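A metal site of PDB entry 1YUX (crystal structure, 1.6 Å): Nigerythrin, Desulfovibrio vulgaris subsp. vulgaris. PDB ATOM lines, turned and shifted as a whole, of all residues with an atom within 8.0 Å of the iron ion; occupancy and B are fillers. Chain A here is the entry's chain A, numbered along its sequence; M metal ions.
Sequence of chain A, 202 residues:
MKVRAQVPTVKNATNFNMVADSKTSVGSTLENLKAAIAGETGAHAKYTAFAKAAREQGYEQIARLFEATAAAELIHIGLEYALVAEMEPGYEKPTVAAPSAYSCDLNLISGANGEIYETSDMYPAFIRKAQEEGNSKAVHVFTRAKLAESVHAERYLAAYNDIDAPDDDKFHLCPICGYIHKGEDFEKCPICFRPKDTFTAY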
ATOM      1  N   ILE A  75      -6.088 -39.281 -20.673  1.00  0.00           N
ATOM      2  CA  ILE A  75      -7.102 -38.391 -21.225  1.00  0.00           C
ATOM      3  C   ILE A  75      -6.773 -38.227 -22.712  1.00  0.00           C
ATOM      4  O   ILE A  75      -7.660 -38.285 -23.563  1.00  0.00           O
ATOM      5  CB  ILE A  75      -7.082 -37.011 -20.527  1.00  0.00           C
ATOM      6  CG1 ILE A  75      -7.672 -37.142 -19.119  1.00  0.00           C
ATOM      7  CG2 ILE A  75      -7.871 -35.989 -21.349  1.00  0.00           C
ATOM      8  CD1 ILE A  75      -7.616 -35.861 -18.311  1.00  0.00           C
ATOM      9  N   ARG A 144      -4.819 -30.002 -28.610  1.00  0.00           N
ATOM     10  CA  ARG A 144      -5.088 -30.073 -27.186  1.00  0.00           C
ATOM     11  C   ARG A 144      -3.991 -30.847 -26.467  1.00  0.00           C
ATOM     12  O   ARG A 144      -3.486 -30.404 -25.437  1.00  0.00           O
ATOM     13  CB  ARG A 144      -6.455 -30.738 -26.955  1.00  0.00           C
ATOM     14  CG  ARG A 144      -6.916 -30.738 -25.513  1.00  0.00           C
ATOM     15  CD  ARG A 144      -8.429 -30.591 -25.427  1.00  0.00           C
ATOM     16  NE  ARG A 144      -8.869 -29.268 -25.863  1.00  0.00           N
ATOM     17  CZ  ARG A 144     -10.110 -28.812 -25.767  1.00  0.00           C
ATOM     18  NH1 ARG A 144     -11.067 -29.587 -25.257  1.00  0.00           N
ATOM     19  NH2 ARG A 144     -10.407 -27.585 -26.169  1.00  0.00           N
ATOM     20  N   ALA A 148      -0.823 -29.496 -23.681  1.00  0.00           N
ATOM     21  CA  ALA A 148      -0.652 -30.052 -22.356  1.00  0.00           C
ATOM     22  C   ALA A 148       0.769 -30.566 -22.116  1.00  0.00           C
ATOM     23  O   ALA A 148       1.301 -30.452 -21.012  1.00  0.00           O
ATOM     24  CB  ALA A 148      -1.645 -31.184 -22.128  1.00  0.00           C
ATOM     25  N   LEU A 173      -5.777 -31.816 -12.213  1.00  0.00           N
ATOM     26  CA  LEU A 173      -5.862 -32.220 -13.611  1.00  0.00           C
ATOM     27  C   LEU A 173      -7.206 -31.847 -14.210  1.00  0.00           C
ATOM     28  O   LEU A 173      -8.258 -32.086 -13.607  1.00  0.00           O
ATOM     29  CB  LEU A 173      -5.665 -33.736 -13.720  1.00  0.00           C
ATOM     30  CG  LEU A 173      -5.792 -34.357 -15.114  1.00  0.00           C
ATOM     31  CD1 LEU A 173      -4.713 -33.773 -16.027  1.00  0.00           C
ATOM     32  CD2 LEU A 173      -5.656 -35.864 -15.006  1.00  0.00           C
ATOM     33  N   CYS A 174      -7.164 -31.258 -15.398  1.00  0.00           N
ATOM     34  CA  CYS A 174      -8.376 -30.862 -16.111  1.00  0.00           C
ATOM     35  C   CYS A 174      -9.160 -32.122 -16.488  1.00  0.00           C
ATOM     36  O   CYS A 174      -8.574 -33.159 -16.739  1.00  0.00           O
ATOM     37  CB  CYS A 174      -7.995 -30.073 -17.369  1.00  0.00           C
ATOM     38  SG  CYS A 174      -9.405 -29.600 -18.401  1.00  0.00           S
ATOM     39  N   PRO A 175     -10.494 -32.026 -16.528  1.00  0.00           N
ATOM     40  CA  PRO A 175     -11.322 -33.184 -16.885  1.00  0.00           C
ATOM     41  C   PRO A 175     -11.284 -33.623 -18.339  1.00  0.00           C
ATOM     42  O   PRO A 175     -11.463 -34.807 -18.638  1.00  0.00           O
ATOM     43  CB  PRO A 175     -12.720 -32.746 -16.453  1.00  0.00           C
ATOM     44  CG  PRO A 175     -12.693 -31.265 -16.679  1.00  0.00           C
ATOM     45  CD  PRO A 175     -11.340 -30.884 -16.112  1.00  0.00           C
ATOM     46  N   ILE A 176     -11.027 -32.688 -19.254  1.00  0.00           N
ATOM     47  CA  ILE A 176     -11.014 -33.027 -20.666  1.00  0.00           C
ATOM     48  C   ILE A 176      -9.710 -32.817 -21.439  1.00  0.00           C
ATOM     49  O   ILE A 176      -9.641 -33.124 -22.632  1.00  0.00           O
ATOM     50  CB  ILE A 176     -12.158 -32.300 -21.414  1.00  0.00           C
ATOM     51  CG1 ILE A 176     -11.943 -30.791 -21.340  1.00  0.00           C
ATOM     52  CG2 ILE A 176     -13.499 -32.679 -20.778  1.00  0.00           C
ATOM     53  CD1 ILE A 176     -12.960 -29.984 -22.144  1.00  0.00           C
ATOM     54  N   CYS A 177      -8.693 -32.287 -20.777  1.00  0.00           N
ATOM     55  CA  CYS A 177      -7.397 -32.107 -21.433  1.00  0.00           C
ATOM     56  C   CYS A 177      -6.321 -32.418 -20.409  1.00  0.00           C
ATOM     57  O   CYS A 177      -6.614 -32.605 -19.222  1.00  0.00           O
ATOM     58  CB  CYS A 177      -7.247 -30.685 -22.011  1.00  0.00           C
ATOM     59  SG  CYS A 177      -6.637 -29.395 -20.917  1.00  0.00           S
ATOM     60  N   GLY A 178      -5.070 -32.481 -20.852  1.00  0.00           N
ATOM     61  CA  GLY A 178      -3.986 -32.826 -19.944  1.00  0.00           C
ATOM     62  C   GLY A 178      -3.419 -31.732 -19.069  1.00  0.00           C
ATOM     63  O   GLY A 178      -2.402 -31.933 -18.410  1.00  0.00           O
ATOM     64  N   TYR A 179      -4.067 -30.575 -19.035  1.00  0.00           N
ATOM     65  CA  TYR A 179      -3.551 -29.486 -18.221  1.00  0.00           C
ATOM     66  C   TYR A 179      -3.473 -29.842 -16.745  1.00  0.00           C
ATOM     67  O   TYR A 179      -4.408 -30.418 -16.187  1.00  0.00           O
ATOM     68  CB  TYR A 179      -4.419 -28.239 -18.381  1.00  0.00           C
ATOM     69  CG  TYR A 179      -3.963 -27.104 -17.498  1.00  0.00           C
ATOM     70  CD1 TYR A 179      -2.774 -26.432 -17.751  1.00  0.00           C
ATOM     71  CD2 TYR A 179      -4.725 -26.719 -16.394  1.00  0.00           C
ATOM     72  CE1 TYR A 179      -2.338 -25.399 -16.918  1.00  0.00           C
ATOM     73  CE2 TYR A 179      -4.297 -25.697 -15.555  1.00  0.00           C
ATOM     74  CZ  TYR A 179      -3.120 -25.035 -15.827  1.00  0.00           C
ATOM     75  OH  TYR A 179      -2.716 -24.004 -15.004  1.00  0.00           O
ATOM     76  N   ILE A 180      -2.359 -29.496 -16.122  1.00  0.00           N
ATOM     77  CA  ILE A 180      -2.139 -29.756 -14.705  1.00  0.00           C
ATOM     78  C   ILE A 180      -1.664 -28.474 -14.042  1.00  0.00           C
ATOM     79  O   ILE A 180      -0.767 -27.803 -14.547  1.00  0.00           O
ATOM     80  CB  ILE A 180      -1.058 -30.827 -14.478  1.00  0.00           C
ATOM     81  CG1 ILE A 180      -1.574 -32.183 -14.952  1.00  0.00           C
ATOM     82  CG2 ILE A 180      -0.661 -30.891 -12.998  1.00  0.00           C
ATOM     83  CD1 ILE A 180      -0.512 -33.266 -14.985  1.00  0.00           C
ATOM     84  N   LYS A 188      -9.350 -21.346 -14.075  1.00  0.00           N
ATOM     85  CA  LYS A 188      -9.795 -22.276 -15.106  1.00  0.00           C
ATOM     86  C   LYS A 188      -8.632 -22.770 -15.943  1.00  0.00           C
ATOM     87  O   LYS A 188      -7.525 -22.240 -15.862  1.00  0.00           O
ATOM     88  CB  LYS A 188     -10.824 -21.600 -16.009  1.00  0.00           C
ATOM     89  CG  LYS A 188     -10.279 -20.390 -16.751  1.00  0.00           C
ATOM     90  CD  LYS A 188     -11.303 -19.829 -17.717  1.00  0.00           C
ATOM     91  CE  LYS A 188     -10.739 -18.626 -18.468  1.00  0.00           C
ATOM     92  NZ  LYS A 188     -11.707 -18.082 -19.467  1.00  0.00           N
ATOM     93  N   CYS A 189      -8.901 -23.792 -16.751  1.00  0.00           N
ATOM     94  CA  CYS A 189      -7.891 -24.380 -17.614  1.00  0.00           C
ATOM     95  C   CYS A 189      -7.538 -23.412 -18.743  1.00  0.00           C
ATOM     96  O   CYS A 189      -8.421 -22.927 -19.445  1.00  0.00           O
ATOM     97  CB  CYS A 189      -8.412 -25.688 -18.202  1.00  0.00           C
ATOM     98  SG  CYS A 189      -7.231 -26.534 -19.272  1.00  0.00           S
ATOM     99  N   PRO A 190      -6.238 -23.112 -18.915  1.00  0.00           N
ATOM    100  CA  PRO A 190      -5.800 -22.188 -19.963  1.00  0.00           C
ATOM    101  C   PRO A 190      -5.819 -22.802 -21.366  1.00  0.00           C
ATOM    102  O   PRO A 190      -5.654 -22.095 -22.367  1.00  0.00           O
ATOM    103  CB  PRO A 190      -4.393 -21.810 -19.521  1.00  0.00           C
ATOM    104  CG  PRO A 190      -3.917 -23.065 -18.872  1.00  0.00           C
ATOM    105  CD  PRO A 190      -5.111 -23.502 -18.060  1.00  0.00           C
ATOM    106  N   ILE A 191      -6.021 -24.115 -21.432  1.00  0.00           N
ATOM    107  CA  ILE A 191      -6.056 -24.817 -22.698  1.00  0.00           C
ATOM    108  C   ILE A 191      -7.483 -24.994 -23.225  1.00  0.00           C
ATOM    109  O   ILE A 191      -7.732 -24.787 -24.413  1.00  0.00           O
ATOM    110  CB  ILE A 191      -5.394 -26.221 -22.581  1.00  0.00           C
ATOM    111  CG1 ILE A 191      -3.896 -26.053 -22.298  1.00  0.00           C
ATOM    112  CG2 ILE A 191      -5.610 -27.014 -23.867  1.00  0.00           C
ATOM    113  CD1 ILE A 191      -3.163 -27.357 -22.063  1.00  0.00           C
ATOM    114  N   CYS A 192      -8.417 -25.354 -22.350  1.00  0.00           N
ATOM    115  CA  CYS A 192      -9.798 -25.554 -22.787  1.00  0.00           C
ATOM    116  C   CYS A 192     -10.825 -24.725 -22.016  1.00  0.00           C
ATOM    117  O   CYS A 192     -12.024 -24.783 -22.306  1.00  0.00           O
ATOM    118  CB  CYS A 192     -10.175 -27.032 -22.677  1.00  0.00           C
ATOM    119  SG  CYS A 192     -10.299 -27.616 -20.980  1.00  0.00           S
ATOM    120  N   PHE A 193     -10.364 -23.957 -21.036  1.00  0.00           N
ATOM    121  CA  PHE A 193     -11.221 -23.082 -20.240  1.00  0.00           C
ATOM    122  C   PHE A 193     -12.137 -23.742 -19.205  1.00  0.00           C
ATOM    123  O   PHE A 193     -12.956 -23.065 -18.578  1.00  0.00           O
ATOM    124  CB  PHE A 193     -12.043 -22.176 -21.160  1.00  0.00           C
ATOM    125  CG  PHE A 193     -11.260 -21.028 -21.741  1.00  0.00           C
ATOM    126  CD1 PHE A 193      -9.863 -21.071 -21.808  1.00  0.00           C
ATOM    127  CD2 PHE A 193     -11.908 -19.903 -22.250  1.00  0.00           C
ATOM    128  CE1 PHE A 193      -9.142 -20.015 -22.363  1.00  0.00           C
ATOM    129  CE2 PHE A 193     -11.201 -18.846 -22.802  1.00  0.00           C
ATOM    130  CZ  PHE A 193      -9.803 -18.895 -22.861  1.00  0.00           C
ATOM    131  N   ARG A 194     -12.010 -25.052 -19.020  1.00  0.00           N
ATOM    132  CA  ARG A 194     -12.824 -25.757 -18.033  1.00  0.00           C
ATOM    133  C   ARG A 194     -12.614 -25.151 -16.649  1.00  0.00           C
ATOM    134  O   ARG A 194     -11.480 -24.878 -16.250  1.00  0.00           O
ATOM    135  CB  ARG A 194     -12.477 -27.238 -17.996  1.00  0.00           C
ATOM    136  CG  ARG A 194     -13.323 -28.113 -18.893  1.00  0.00           C
ATOM    137  CD  ARG A 194     -14.760 -28.160 -18.384  1.00  0.00           C
ATOM    138  NE  ARG A 194     -15.558 -29.159 -19.091  1.00  0.00           N
ATOM    139  CZ  ARG A 194     -15.969 -29.050 -20.346  1.00  0.00           C
ATOM    140  NH1 ARG A 194     -15.671 -27.966 -21.063  1.00  0.00           N
ATOM    141  NH2 ARG A 194     -16.688 -30.018 -20.901  1.00  0.00           N
ATOM    142  N   PRO A 195     -13.704 -24.912 -15.903  1.00  0.00           N
ATOM    143  CA  PRO A 195     -13.621 -24.333 -14.560  1.00  0.00           C
ATOM    144  C   PRO A 195     -12.836 -25.206 -13.586  1.00  0.00           C
ATOM    145  O   PRO A 195     -12.821 -26.430 -13.701  1.00  0.00           O
ATOM    146  CB  PRO A 195     -15.076 -24.191 -14.156  1.00  0.00           C
ATOM    147  CG  PRO A 195     -15.769 -23.966 -15.461  1.00  0.00           C
ATOM    148  CD  PRO A 195     -15.104 -25.000 -16.341  1.00  0.00           C
ATOM    149  N   THR A 198     -14.103 -28.477 -11.854  1.00  0.00           N
ATOM    150  CA  THR A 198     -14.312 -29.703 -12.623  1.00  0.00           C
ATOM    151  C   THR A 198     -13.043 -30.557 -12.673  1.00  0.00           C
ATOM    152  O   THR A 198     -13.048 -31.656 -13.222  1.00  0.00           O
ATOM    153  CB  THR A 198     -14.757 -29.396 -14.064  1.00  0.00           C
ATOM    154  OG1 THR A 198     -13.690 -28.757 -14.780  1.00  0.00           O
ATOM    155  CG2 THR A 198     -15.973 -28.483 -14.064  1.00  0.00           C
ATOM    156  N   PHE A 199     -11.969 -30.043 -12.082  1.00  0.00           N
ATOM    157  CA  PHE A 199     -10.692 -30.737 -12.036  1.00  0.00           C
ATOM    158  C   PHE A 199     -10.674 -31.852 -11.005  1.00  0.00           C
ATOM    159  O   PHE A 199     -11.570 -31.972 -10.167  1.00  0.00           O
ATOM    160  CB  PHE A 199      -9.566 -29.749 -11.697  1.00  0.00           C
ATOM    161  CG  PHE A 199      -9.105 -28.889 -12.848  1.00  0.00           C
ATOM    162  CD1 PHE A 199     -10.015 -28.152 -13.593  1.00  0.00           C
ATOM    163  CD2 PHE A 199      -7.751 -28.790 -13.155  1.00  0.00           C
ATOM    164  CE1 PHE A 199      -9.575 -27.321 -14.625  1.00  0.00           C
ATOM    165  CE2 PHE A 199      -7.305 -27.972 -14.184  1.00  0.00           C
ATOM    166  CZ  PHE A 199      -8.220 -27.228 -14.924  1.00  0.00           C
HETATM  167 FE    FE M   1      -8.418 -28.345 -20.004  1.00  0.00          FE
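Within 4 Å of the iron ion: Cys 174, Cys 177, Cys 189 and Cys 192.
SG of Cys 192 is bound to the iron ion (2.2 Å).
The iron ion is bound by SG of Cys 177 (2.3 Å).
The iron ion is bound by SG of Cys 174 (2.3 Å).
SG of Cys 189 is bound to the iron ion, 2.3 Å away.
The iron ion has four donor atoms within binding distance.
The backbone NH of Arg 194 lies close to the side-chain sulfur of Cys 192 (3.7 Å).
SG of Cys 177 lies close to N of Tyr 179 (3.4 Å).
The backbone carbonyl oxygen of Tyr 179 sits at hydrogen-bond distance from the backbone NH of Cys 174, at 3.0 Å.
The backbone NH of Ile 176 lies close to the side-chain sulfur of Cys 174, at 3.6 Å.
The side-chain sulfur of Cys 189 lies close to the backbone NH of Ile 191, 3.5 Å away.
The backbone carbonyl oxygen of Arg 194 sits at hydrogen-bond distance from the backbone NH of Cys 189, at 2.8 Å.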
